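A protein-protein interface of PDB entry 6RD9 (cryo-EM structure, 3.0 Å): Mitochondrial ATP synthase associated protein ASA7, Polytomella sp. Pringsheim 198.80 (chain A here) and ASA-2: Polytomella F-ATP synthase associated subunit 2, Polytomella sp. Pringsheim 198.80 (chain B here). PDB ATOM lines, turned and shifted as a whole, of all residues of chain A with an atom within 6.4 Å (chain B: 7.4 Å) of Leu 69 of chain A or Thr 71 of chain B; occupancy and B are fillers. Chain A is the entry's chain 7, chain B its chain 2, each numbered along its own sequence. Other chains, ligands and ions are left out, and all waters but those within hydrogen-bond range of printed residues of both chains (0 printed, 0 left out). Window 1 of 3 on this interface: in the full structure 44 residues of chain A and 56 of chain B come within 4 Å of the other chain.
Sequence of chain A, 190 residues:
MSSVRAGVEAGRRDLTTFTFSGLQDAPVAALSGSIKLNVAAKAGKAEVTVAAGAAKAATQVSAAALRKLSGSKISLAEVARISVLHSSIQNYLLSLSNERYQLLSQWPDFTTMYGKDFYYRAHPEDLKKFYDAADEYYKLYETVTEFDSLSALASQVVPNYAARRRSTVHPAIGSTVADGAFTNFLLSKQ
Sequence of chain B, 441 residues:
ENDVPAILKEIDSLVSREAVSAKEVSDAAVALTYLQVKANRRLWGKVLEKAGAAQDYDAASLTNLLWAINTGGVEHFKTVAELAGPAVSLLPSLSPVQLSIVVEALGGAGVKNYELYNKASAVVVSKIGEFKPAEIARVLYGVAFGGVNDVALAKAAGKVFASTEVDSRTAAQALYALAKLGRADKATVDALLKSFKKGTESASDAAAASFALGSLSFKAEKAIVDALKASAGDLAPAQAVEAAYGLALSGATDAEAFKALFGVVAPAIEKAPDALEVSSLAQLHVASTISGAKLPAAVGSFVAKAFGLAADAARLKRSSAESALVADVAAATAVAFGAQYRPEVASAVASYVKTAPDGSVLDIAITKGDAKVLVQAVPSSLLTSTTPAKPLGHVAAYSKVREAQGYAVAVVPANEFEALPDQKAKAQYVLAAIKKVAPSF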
ATOM      1  N   LEU A  15      10.461  12.617  -8.813  1.00  0.00           N
ATOM      2  CA  LEU A  15      11.079  11.380  -8.382  1.00  0.00           C
ATOM      3  C   LEU A  15      12.520  11.322  -8.821  1.00  0.00           C
ATOM      4  O   LEU A  15      12.903  11.957  -9.793  1.00  0.00           O
ATOM      5  CB  LEU A  15      10.315  10.185  -8.925  1.00  0.00           C
ATOM      6  CG  LEU A  15       9.451   9.464  -7.911  1.00  0.00           C
ATOM      7  CD1 LEU A  15       8.820   8.297  -8.575  1.00  0.00           C
ATOM      8  CD2 LEU A  15      10.315   8.994  -6.777  1.00  0.00           C
ATOM      9  N   THR A  19      14.878   4.096  -7.503  1.00  0.00           N
ATOM     10  CA  THR A  19      13.915   3.935  -6.429  1.00  0.00           C
ATOM     11  C   THR A  19      14.101   2.552  -5.822  1.00  0.00           C
ATOM     12  O   THR A  19      14.387   1.588  -6.534  1.00  0.00           O
ATOM     13  CB  THR A  19      12.499   4.124  -6.963  1.00  0.00           C
ATOM     14  OG1 THR A  19      12.434   5.356  -7.683  1.00  0.00           O
ATOM     15  CG2 THR A  19      11.499   4.203  -5.844  1.00  0.00           C
ATOM     16  N   SER A  21      11.919   0.655  -3.640  1.00  0.00           N
ATOM     17  CA  SER A  21      10.748   0.060  -3.025  1.00  0.00           C
ATOM     18  C   SER A  21      10.101  -0.906  -4.001  1.00  0.00           C
ATOM     19  O   SER A  21      10.227  -0.772  -5.217  1.00  0.00           O
ATOM     20  CB  SER A  21       9.738   1.113  -2.593  1.00  0.00           C
ATOM     21  OG  SER A  21       9.036   1.600  -3.711  1.00  0.00           O
ATOM     22  N   GLY A  22       9.402  -1.886  -3.439  1.00  0.00           N
ATOM     23  CA  GLY A  22       8.685  -2.874  -4.216  1.00  0.00           C
ATOM     24  C   GLY A  22       8.840  -4.283  -3.684  1.00  0.00           C
ATOM     25  O   GLY A  22       9.954  -4.798  -3.580  1.00  0.00           O
ATOM     26  N   LEU A  23       7.714  -4.901  -3.334  1.00  0.00           N
ATOM     27  CA  LEU A  23       7.569  -6.261  -2.813  1.00  0.00           C
ATOM     28  C   LEU A  23       8.355  -6.538  -1.541  1.00  0.00           C
ATOM     29  O   LEU A  23       8.500  -7.698  -1.164  1.00  0.00           O
ATOM     30  CB  LEU A  23       7.922  -7.317  -3.859  1.00  0.00           C
ATOM     31  CG  LEU A  23       6.845  -7.652  -4.883  1.00  0.00           C
ATOM     32  CD1 LEU A  23       7.135  -8.993  -5.503  1.00  0.00           C
ATOM     33  CD2 LEU A  23       5.458  -7.648  -4.270  1.00  0.00           C
ATOM     34  N   ALA A  65      10.325  -7.228 -10.904  1.00  0.00           N
ATOM     35  CA  ALA A  65       9.375  -6.664 -11.850  1.00  0.00           C
ATOM     36  C   ALA A  65       8.759  -5.377 -11.346  1.00  0.00           C
ATOM     37  O   ALA A  65       8.391  -4.522 -12.153  1.00  0.00           O
ATOM     38  CB  ALA A  65       8.262  -7.663 -12.165  1.00  0.00           C
ATOM     39  N   LEU A  66       8.641  -5.226 -10.031  1.00  0.00           N
ATOM     40  CA  LEU A  66       8.255  -3.953  -9.454  1.00  0.00           C
ATOM     41  C   LEU A  66       9.391  -2.947  -9.439  1.00  0.00           C
ATOM     42  O   LEU A  66       9.134  -1.743  -9.352  1.00  0.00           O
ATOM     43  CB  LEU A  66       7.750  -4.147  -8.031  1.00  0.00           C
ATOM     44  CG  LEU A  66       6.327  -4.651  -7.852  1.00  0.00           C
ATOM     45  CD1 LEU A  66       5.882  -4.305  -6.463  1.00  0.00           C
ATOM     46  CD2 LEU A  66       5.399  -4.048  -8.874  1.00  0.00           C
ATOM     47  N   ARG A  67      10.635  -3.402  -9.511  1.00  0.00           N
ATOM     48  CA  ARG A  67      11.739  -2.459  -9.513  1.00  0.00           C
ATOM     49  C   ARG A  67      11.931  -1.828 -10.875  1.00  0.00           C
ATOM     50  O   ARG A  67      12.450  -0.716 -10.966  1.00  0.00           O
ATOM     51  CB  ARG A  67      13.015  -3.149  -9.064  1.00  0.00           C
ATOM     52  CG  ARG A  67      12.916  -3.747  -7.698  1.00  0.00           C
ATOM     53  CD  ARG A  67      12.919  -2.691  -6.633  1.00  0.00           C
ATOM     54  NE  ARG A  67      14.011  -1.752  -6.832  1.00  0.00           N
ATOM     55  CZ  ARG A  67      15.269  -1.974  -6.467  1.00  0.00           C
ATOM     56  NH1 ARG A  67      15.609  -3.110  -5.881  1.00  0.00           N
ATOM     57  NH2 ARG A  67      16.194  -1.055  -6.693  1.00  0.00           N
ATOM     58  N   LYS A  68      11.515  -2.499 -11.936  1.00  0.00           N
ATOM     59  CA  LYS A  68      11.537  -1.874 -13.247  1.00  0.00           C
ATOM     60  C   LYS A  68      10.362  -0.947 -13.476  1.00  0.00           C
ATOM     61  O   LYS A  68      10.291  -0.323 -14.539  1.00  0.00           O
ATOM     62  CB  LYS A  68      11.539  -2.923 -14.350  1.00  0.00           C
ATOM     63  CG  LYS A  68      12.593  -3.972 -14.220  1.00  0.00           C
ATOM     64  CD  LYS A  68      12.648  -4.787 -15.492  1.00  0.00           C
ATOM     65  CE  LYS A  68      13.390  -6.079 -15.287  1.00  0.00           C
ATOM     66  NZ  LYS A  68      13.769  -6.664 -16.590  1.00  0.00           N
ATOM     67  N   LEU A  69       9.430  -0.864 -12.528  1.00  0.00           N
ATOM     68  CA  LEU A  69       8.250  -0.036 -12.732  1.00  0.00           C
ATOM     69  C   LEU A  69       8.591   1.436 -12.634  1.00  0.00           C
ATOM     70  O   LEU A  69       8.133   2.242 -13.448  1.00  0.00           O
ATOM     71  CB  LEU A  69       7.180  -0.409 -11.719  1.00  0.00           C
ATOM     72  CG  LEU A  69       5.750  -0.215 -12.188  1.00  0.00           C
ATOM     73  CD1 LEU A  69       5.544  -0.920 -13.478  1.00  0.00           C
ATOM     74  CD2 LEU A  69       4.844  -0.761 -11.144  1.00  0.00           C
ATOM     75  N   SER A  70       9.440   1.798 -11.681  1.00  0.00           N
ATOM     76  CA  SER A  70       9.868   3.171 -11.485  1.00  0.00           C
ATOM     77  C   SER A  70      11.060   3.536 -12.339  1.00  0.00           C
ATOM     78  O   SER A  70      11.887   4.343 -11.915  1.00  0.00           O
ATOM     79  CB  SER A  70      10.201   3.398 -10.017  1.00  0.00           C
ATOM     80  OG  SER A  70      11.330   2.639  -9.668  1.00  0.00           O
ATOM     81  N   GLY A  71      11.199   2.937 -13.512  1.00  0.00           N
ATOM     82  CA  GLY A  71      12.310   3.236 -14.383  1.00  0.00           C
ATOM     83  C   GLY A  71      11.981   4.362 -15.325  1.00  0.00           C
ATOM     84  O   GLY A  71      12.758   5.305 -15.472  1.00  0.00           O
ATOM     85  N   SER A  72      10.842   4.258 -15.992  1.00  0.00           N
ATOM     86  CA  SER A  72      10.307   5.342 -16.798  1.00  0.00           C
ATOM     87  C   SER A  72       9.140   5.953 -16.041  1.00  0.00           C
ATOM     88  O   SER A  72       8.143   5.278 -15.791  1.00  0.00           O
ATOM     89  CB  SER A  72       9.867   4.837 -18.167  1.00  0.00           C
ATOM     90  OG  SER A  72       9.082   3.673 -18.034  1.00  0.00           O
ATOM     91  N   LYS A  73       9.267   7.219 -15.676  1.00  0.00           N
ATOM     92  CA  LYS A  73       8.314   7.840 -14.779  1.00  0.00           C
ATOM     93  C   LYS A  73       7.049   8.246 -15.519  1.00  0.00           C
ATOM     94  O   LYS A  73       7.057   8.443 -16.735  1.00  0.00           O
ATOM     95  CB  LYS A  73       8.933   9.059 -14.113  1.00  0.00           C
ATOM     96  CG  LYS A  73      10.245   8.786 -13.429  1.00  0.00           C
ATOM     97  CD  LYS A  73      10.035   8.197 -12.076  1.00  0.00           C
ATOM     98  CE  LYS A  73      11.309   7.584 -11.552  1.00  0.00           C
ATOM     99  NZ  LYS A  73      12.485   8.360 -11.968  1.00  0.00           N
ATOM    100  N   LEU B  32      -2.850  -0.527  -8.834  1.00  0.00           N
ATOM    101  CA  LEU B  32      -2.340  -0.107 -10.129  1.00  0.00           C
ATOM    102  C   LEU B  32      -0.845  -0.327 -10.262  1.00  0.00           C
ATOM    103  O   LEU B  32      -0.323  -0.288 -11.375  1.00  0.00           O
ATOM    104  CB  LEU B  32      -2.669   1.359 -10.374  1.00  0.00           C
ATOM    105  CG  LEU B  32      -4.093   1.755 -10.726  1.00  0.00           C
ATOM    106  CD1 LEU B  32      -4.213   3.231 -10.776  1.00  0.00           C
ATOM    107  CD2 LEU B  32      -4.456   1.198 -12.040  1.00  0.00           C
ATOM    108  N   THR B  33      -0.136  -0.534  -9.162  1.00  0.00           N
ATOM    109  CA  THR B  33       1.273  -0.875  -9.264  1.00  0.00           C
ATOM    110  C   THR B  33       1.478  -2.369  -9.403  1.00  0.00           C
ATOM    111  O   THR B  33       2.264  -2.801 -10.248  1.00  0.00           O
ATOM    112  CB  THR B  33       2.031  -0.367  -8.051  1.00  0.00           C
ATOM    113  OG1 THR B  33       1.687  -1.155  -6.914  1.00  0.00           O
ATOM    114  CG2 THR B  33       1.639   1.027  -7.784  1.00  0.00           C
ATOM    115  N   TYR B  34       0.746  -3.169  -8.616  1.00  0.00           N
ATOM    116  CA  TYR B  34       0.764  -4.621  -8.745  1.00  0.00           C
ATOM    117  C   TYR B  34       0.287  -5.086 -10.106  1.00  0.00           C
ATOM    118  O   TYR B  34       0.638  -6.184 -10.531  1.00  0.00           O
ATOM    119  CB  TYR B  34      -0.127  -5.250  -7.697  1.00  0.00           C
ATOM    120  CG  TYR B  34       0.445  -5.313  -6.323  1.00  0.00           C
ATOM    121  CD1 TYR B  34      -0.337  -5.027  -5.229  1.00  0.00           C
ATOM    122  CD2 TYR B  34       1.744  -5.700  -6.111  1.00  0.00           C
ATOM    123  CE1 TYR B  34       0.163  -5.094  -3.967  1.00  0.00           C
ATOM    124  CE2 TYR B  34       2.256  -5.774  -4.846  1.00  0.00           C
ATOM    125  CZ  TYR B  34       1.454  -5.471  -3.778  1.00  0.00           C
ATOM    126  OH  TYR B  34       1.944  -5.535  -2.501  1.00  0.00           O
ATOM    127  N   LEU B  35      -0.501  -4.281 -10.793  1.00  0.00           N
ATOM    128  CA  LEU B  35      -0.925  -4.569 -12.143  1.00  0.00           C
ATOM    129  C   LEU B  35      -0.035  -3.919 -13.187  1.00  0.00           C
ATOM    130  O   LEU B  35      -0.203  -4.218 -14.374  1.00  0.00           O
ATOM    131  CB  LEU B  35      -2.355  -4.086 -12.350  1.00  0.00           C
ATOM    132  CG  LEU B  35      -3.559  -4.991 -12.156  1.00  0.00           C
ATOM    133  CD1 LEU B  35      -3.518  -5.644 -10.810  1.00  0.00           C
ATOM    134  CD2 LEU B  35      -4.791  -4.144 -12.278  1.00  0.00           C
ATOM    135  N   GLN B  36       0.874  -3.026 -12.769  1.00  0.00           N
ATOM    136  CA  GLN B  36       1.904  -2.403 -13.608  1.00  0.00           C
ATOM    137  C   GLN B  36       1.297  -1.610 -14.773  1.00  0.00           C
ATOM    138  O   GLN B  36       1.407  -1.981 -15.938  1.00  0.00           O
ATOM    139  CB  GLN B  36       2.894  -3.455 -14.108  1.00  0.00           C
ATOM    140  CG  GLN B  36       3.498  -4.281 -13.006  1.00  0.00           C
ATOM    141  CD  GLN B  36       4.415  -5.337 -13.542  1.00  0.00           C
ATOM    142  OE1 GLN B  36       5.193  -5.093 -14.462  1.00  0.00           O
ATOM    143  NE2 GLN B  36       4.313  -6.533 -12.992  1.00  0.00           N
ATOM    144  N   VAL B  37       0.669  -0.485 -14.418  1.00  0.00           N
ATOM    145  CA  VAL B  37      -0.251   0.238 -15.295  1.00  0.00           C
ATOM    146  C   VAL B  37       0.422   1.547 -15.719  1.00  0.00           C
ATOM    147  O   VAL B  37      -0.122   2.643 -15.554  1.00  0.00           O
ATOM    148  CB  VAL B  37      -1.625   0.441 -14.619  1.00  0.00           C
ATOM    149  CG1 VAL B  37      -2.699   0.905 -15.608  1.00  0.00           C
ATOM    150  CG2 VAL B  37      -2.090  -0.834 -14.041  1.00  0.00           C
ATOM    151  N   LYS B  38       1.681   1.465 -16.134  1.00  0.00           N
ATOM    152  CA  LYS B  38       2.338   2.648 -16.678  1.00  0.00           C
ATOM    153  C   LYS B  38       1.725   3.149 -17.979  1.00  0.00           C
ATOM    154  O   LYS B  38       1.948   4.306 -18.339  1.00  0.00           O
ATOM    155  CB  LYS B  38       3.811   2.377 -16.922  1.00  0.00           C
ATOM    156  CG  LYS B  38       4.476   1.724 -15.775  1.00  0.00           C
ATOM    157  CD  LYS B  38       4.522   2.638 -14.589  1.00  0.00           C
ATOM    158  CE  LYS B  38       5.407   3.809 -14.861  1.00  0.00           C
ATOM    159  NZ  LYS B  38       6.761   3.386 -15.251  1.00  0.00           N
ATOM    160  N   TRP B  44      -4.025   6.830 -13.683  1.00  0.00           N
ATOM    161  CA  TRP B  44      -3.187   7.248 -12.574  1.00  0.00           C
ATOM    162  C   TRP B  44      -3.474   8.684 -12.193  1.00  0.00           C
ATOM    163  O   TRP B  44      -3.255   9.074 -11.045  1.00  0.00           O
ATOM    164  CB  TRP B  44      -1.724   7.091 -12.930  1.00  0.00           C
ATOM    165  CG  TRP B  44      -1.084   5.885 -12.400  1.00  0.00           C
ATOM    166  CD1 TRP B  44      -0.592   4.860 -13.118  1.00  0.00           C
ATOM    167  CD2 TRP B  44      -0.838   5.576 -11.031  1.00  0.00           C
ATOM    168  NE1 TRP B  44      -0.056   3.920 -12.290  1.00  0.00           N
ATOM    169  CE2 TRP B  44      -0.195   4.341 -10.998  1.00  0.00           C
ATOM    170  CE3 TRP B  44      -1.108   6.219  -9.829  1.00  0.00           C
ATOM    171  CZ2 TRP B  44       0.190   3.744  -9.823  1.00  0.00           C
ATOM    172  CZ3 TRP B  44      -0.730   5.619  -8.664  1.00  0.00           C
ATOM    173  CH2 TRP B  44      -0.086   4.402  -8.667  1.00  0.00           C
ATOM    174  N   LEU B  65      -0.609   4.349   0.068  1.00  0.00           N
ATOM    175  CA  LEU B  65      -0.665   5.249  -1.069  1.00  0.00           C
ATOM    176  C   LEU B  65       0.725   5.693  -1.469  1.00  0.00           C
ATOM    177  O   LEU B  65       1.083   5.632  -2.647  1.00  0.00           O
ATOM    178  CB  LEU B  65      -1.524   6.454  -0.734  1.00  0.00           C
ATOM    179  CG  LEU B  65      -1.631   7.487  -1.828  1.00  0.00           C
ATOM    180  CD1 LEU B  65      -2.409   6.929  -2.960  1.00  0.00           C
ATOM    181  CD2 LEU B  65      -2.337   8.639  -1.264  1.00  0.00           C
ATOM    182  N   LEU B  66       1.531   6.106  -0.492  1.00  0.00           N
ATOM    183  CA  LEU B  66       2.856   6.630  -0.774  1.00  0.00           C
ATOM    184  C   LEU B  66       3.795   5.546  -1.261  1.00  0.00           C
ATOM    185  O   LEU B  66       4.698   5.834  -2.047  1.00  0.00           O
ATOM    186  CB  LEU B  66       3.412   7.309   0.464  1.00  0.00           C
ATOM    187  CG  LEU B  66       2.894   8.722   0.642  1.00  0.00           C
ATOM    188  CD1 LEU B  66       3.416   9.304   1.902  1.00  0.00           C
ATOM    189  CD2 LEU B  66       3.310   9.570  -0.508  1.00  0.00           C
ATOM    190  N   TRP B  67       3.590   4.303  -0.826  1.00  0.00           N
ATOM    191  CA  TRP B  67       4.305   3.181  -1.420  1.00  0.00           C
ATOM    192  C   TRP B  67       3.958   3.035  -2.885  1.00  0.00           C
ATOM    193  O   TRP B  67       4.837   2.799  -3.709  1.00  0.00           O
ATOM    194  CB  TRP B  67       3.976   1.883  -0.690  1.00  0.00           C
ATOM    195  CG  TRP B  67       4.624   0.678  -1.278  1.00  0.00           C
ATOM    196  CD1 TRP B  67       5.841   0.192  -0.969  1.00  0.00           C
ATOM    197  CD2 TRP B  67       4.089  -0.190  -2.277  1.00  0.00           C
ATOM    198  NE1 TRP B  67       6.110  -0.915  -1.711  1.00  0.00           N
ATOM    199  CE2 TRP B  67       5.047  -1.168  -2.529  1.00  0.00           C
ATOM    200  CE3 TRP B  67       2.890  -0.230  -2.987  1.00  0.00           C
ATOM    201  CZ2 TRP B  67       4.851  -2.172  -3.452  1.00  0.00           C
ATOM    202  CZ3 TRP B  67       2.704  -1.221  -3.905  1.00  0.00           C
ATOM    203  CH2 TRP B  67       3.673  -2.176  -4.130  1.00  0.00           C
ATOM    204  N   ALA B  68       2.686   3.188  -3.230  1.00  0.00           N
ATOM    205  CA  ALA B  68       2.259   2.943  -4.599  1.00  0.00           C
ATOM    206  C   ALA B  68       2.696   4.058  -5.527  1.00  0.00           C
ATOM    207  O   ALA B  68       2.960   3.819  -6.706  1.00  0.00           O
ATOM    208  CB  ALA B  68       0.752   2.782  -4.638  1.00  0.00           C
ATOM    209  N   ILE B  69       2.762   5.282  -5.015  1.00  0.00           N
ATOM    210  CA  ILE B  69       3.269   6.401  -5.797  1.00  0.00           C
ATOM    211  C   ILE B  69       4.751   6.217  -6.074  1.00  0.00           C
ATOM    212  O   ILE B  69       5.212   6.379  -7.206  1.00  0.00           O
ATOM    213  CB  ILE B  69       2.989   7.712  -5.048  1.00  0.00           C
ATOM    214  CG1 ILE B  69       1.497   7.985  -4.978  1.00  0.00           C
ATOM    215  CG2 ILE B  69       3.672   8.858  -5.702  1.00  0.00           C
ATOM    216  CD1 ILE B  69       1.158   9.073  -4.033  1.00  0.00           C
ATOM    217  N   ASN B  70       5.505   5.815  -5.055  1.00  0.00           N
ATOM    218  CA  ASN B  70       6.942   5.646  -5.187  1.00  0.00           C
ATOM    219  C   ASN B  70       7.291   4.444  -6.046  1.00  0.00           C
ATOM    220  O   ASN B  70       8.121   4.548  -6.949  1.00  0.00           O
ATOM    221  CB  ASN B  70       7.556   5.495  -3.812  1.00  0.00           C
ATOM    222  CG  ASN B  70       8.997   5.813  -3.808  1.00  0.00           C
ATOM    223  OD1 ASN B  70       9.436   6.730  -4.487  1.00  0.00           O
ATOM    224  ND2 ASN B  70       9.767   5.054  -3.048  1.00  0.00           N
ATOM    225  N   THR B  71       6.674   3.295  -5.776  1.00  0.00           N
ATOM    226  CA  THR B  71       6.981   2.080  -6.519  1.00  0.00           C
ATOM    227  C   THR B  71       6.488   2.165  -7.950  1.00  0.00           C
ATOM    228  O   THR B  71       7.156   1.689  -8.871  1.00  0.00           O
ATOM    229  CB  THR B  71       6.359   0.888  -5.821  1.00  0.00           C
ATOM    230  OG1 THR B  71       6.735   0.915  -4.447  1.00  0.00           O
ATOM    231  CG2 THR B  71       6.816  -0.396  -6.428  1.00  0.00           C
ATOM    232  N   GLY B  72       5.337   2.784  -8.164  1.00  0.00           N
ATOM    233  CA  GLY B  72       4.817   2.873  -9.504  1.00  0.00           C
ATOM    234  C   GLY B  72       5.548   3.840 -10.387  1.00  0.00           C
ATOM    235  O   GLY B  72       5.353   3.803 -11.603  1.00  0.00           O
ATOM    236  N   GLY B  73       6.378   4.699  -9.816  1.00  0.00           N
ATOM    237  CA  GLY B  73       7.116   5.657 -10.605  1.00  0.00           C
ATOM    238  C   GLY B  73       6.292   6.816 -11.078  1.00  0.00           C
ATOM    239  O   GLY B  73       6.639   7.451 -12.064  1.00  0.00           O
ATOM    240  N   VAL B  74       5.188   7.100 -10.420  1.00  0.00           N
ATOM    241  CA  VAL B  74       4.311   8.189 -10.813  1.00  0.00           C
ATOM    242  C   VAL B  74       4.669   9.394  -9.966  1.00  0.00           C
ATOM    243  O   VAL B  74       4.833   9.283  -8.749  1.00  0.00           O
ATOM    244  CB  VAL B  74       2.832   7.783 -10.676  1.00  0.00           C
ATOM    245  CG1 VAL B  74       2.593   7.083  -9.386  1.00  0.00           C
ATOM    246  CG2 VAL B  74       1.935   8.968 -10.762  1.00  0.00           C
ATOM    247  N   ILE B 101       8.409   4.220   4.892  1.00  0.00           N
ATOM    248  CA  ILE B 101       7.802   4.326   3.569  1.00  0.00           C
ATOM    249  C   ILE B 101       7.324   5.747   3.305  1.00  0.00           C
ATOM    250  O   ILE B 101       7.378   6.222   2.168  1.00  0.00           O
ATOM    251  CB  ILE B 101       6.662   3.308   3.424  1.00  0.00           C
ATOM    252  CG1 ILE B 101       7.136   1.905   3.794  1.00  0.00           C
ATOM    253  CG2 ILE B 101       6.116   3.290   2.012  1.00  0.00           C
ATOM    254  CD1 ILE B 101       8.052   1.273   2.783  1.00  0.00           C
ATOM    255  N   GLU B 104      10.591   7.897   2.711  1.00  0.00           N
ATOM    256  CA  GLU B 104      11.212   7.547   1.438  1.00  0.00           C
ATOM    257  C   GLU B 104      10.408   8.074   0.265  1.00  0.00           C
ATOM    258  O   GLU B 104      10.979   8.521  -0.731  1.00  0.00           O
ATOM    259  CB  GLU B 104      11.368   6.043   1.301  1.00  0.00           C
ATOM    260  CG  GLU B 104      12.164   5.646   0.100  1.00  0.00           C
ATOM    261  CD  GLU B 104      11.701   4.370  -0.540  1.00  0.00           C
ATOM    262  OE1 GLU B 104      10.631   3.861  -0.158  1.00  0.00           O
ATOM    263  OE2 GLU B 104      12.406   3.887  -1.446  1.00  0.00           O
ATOM    264  N   ALA B 105       9.085   8.044   0.362  1.00  0.00           N
ATOM    265  CA  ALA B 105       8.268   8.498  -0.753  1.00  0.00           C
ATOM    266  C   ALA B 105       8.188  10.012  -0.804  1.00  0.00           C
ATOM    267  O   ALA B 105       8.222  10.600  -1.885  1.00  0.00           O
ATOM    268  CB  ALA B 105       6.881   7.892  -0.656  1.00  0.00           C
ATOM    269  N   SER B 204      18.792  -2.160 -10.583  1.00  0.00           N
ATOM    270  CA  SER B 204      18.631  -0.784 -10.157  1.00  0.00           C
ATOM    271  C   SER B 204      19.464  -0.493  -8.924  1.00  0.00           C
ATOM    272  O   SER B 204      19.866   0.650  -8.710  1.00  0.00           O
ATOM    273  CB  SER B 204      17.159  -0.492  -9.904  1.00  0.00           C
ATOM    274  OG  SER B 204      16.415  -0.656 -11.097  1.00  0.00           O
ATOM    275  N   ASP B 234      17.699  -4.494 -17.637  1.00  0.00           N
ATOM    276  CA  ASP B 234      16.725  -4.135 -16.624  1.00  0.00           C
ATOM    277  C   ASP B 234      16.661  -2.639 -16.393  1.00  0.00           C
ATOM    278  O   ASP B 234      15.730  -2.165 -15.735  1.00  0.00           O
ATOM    279  CB  ASP B 234      17.067  -4.818 -15.300  1.00  0.00           C
ATOM    280  CG  ASP B 234      16.967  -6.323 -15.370  1.00  0.00           C
ATOM    281  OD1 ASP B 234      17.079  -6.971 -14.308  1.00  0.00           O
ATOM    282  OD2 ASP B 234      16.784  -6.864 -16.478  1.00  0.00           O
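NZ of Lys 38 of chain B is in hydrogen-bond range of O of Ser 72 of chain A (2.4 Å).
OG1 of Thr 71 of chain B lies within hydrogen-bond range of OG of Ser 21 of chain A (2.5 Å).
The backbone carbonyl oxygen of Leu 69 of chain A is in hydrogen-bond range of the side-chain amino group of Lys 38 of chain B.
OD2 of Asp 234 of chain B is in salt-bridge range of NZ of Lys 68 of chain A, 3.0 Å away.
The side-chain amide nitrogen (ND2) of Asn 70 of chain B lies close to the side-chain carboxylate (OE1) of Glu 104 of chain B.
O of Trp 67 of chain B sits at hydrogen-bond distance from OG1 of Thr 71 of chain B (2.8 Å).
The backbone carbonyl oxygen of Thr 19 of chain A sits at hydrogen-bond distance from the guanidinium group of Arg 67 of chain A (3.2 Å).
Leu 15 of chain A touches Asn 70 of chain B.
CG2 of Thr 19 of chain A touches ND2 of Asn 70 of chain B, 3.4 Å away.
OG of Ser 21 of chain A touches ND2 of Asn 70 of chain B, 3.6 Å away.
Leu 23 of chain A touches Tyr 34 of chain B (CD2 to CE2, 3.8 Å).
Leu 23 of chain A touches Trp 67 of chain B.
Ala 65 of chain A touches Gln 36 of chain B.
Leu 66 of chain A touches Trp 67 of chain B.
CD2 of Leu 69 of chain A touches O of Thr 33 of chain B, 3.4 Å away.
O of Gly 72 of chain B touches O of Leu 69 of chain A, at 3.7 Å.
Asn 70 of chain B touches Ser 70 of chain A.
Printed residues of chain B within 4 Å of Gly 22 of chain A: Trp 67 and Thr 71.
Leu 69 of chain A touches just these residues of chain B: Thr 33, Gln 36, Lys 38, Thr 71 and Gly 72.
Ala 68 of chain B touches none of the printed residues of chain A.
Of chain A, only Ser 21, Gly 22, Leu 66, Leu 69 and Ser 70 come within 4 Å of Thr 71 of chain B.
Printed residues of chain A within 4 Å of Gly 72 of chain B: Leu 69 (3.7 Å).
Of the printed residues of chain A, Ser 204 of chain B touches Arg 67.
The nearest printed residue of chain B that does not touch Arg 67 of chain A is Thr 71 of chain B (5.8 Å).
Hydrophobic or aromatic side chains of chain B that line the printed part of chain A: Tyr 34 and Trp 67.
Among the printed residues, Asp or Glu carboxylates within 4 Å of a Lys or Arg side-chain nitrogen of the other chain: Lys 68 of chain A with Asp 234 of chain B (3.0 Å).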
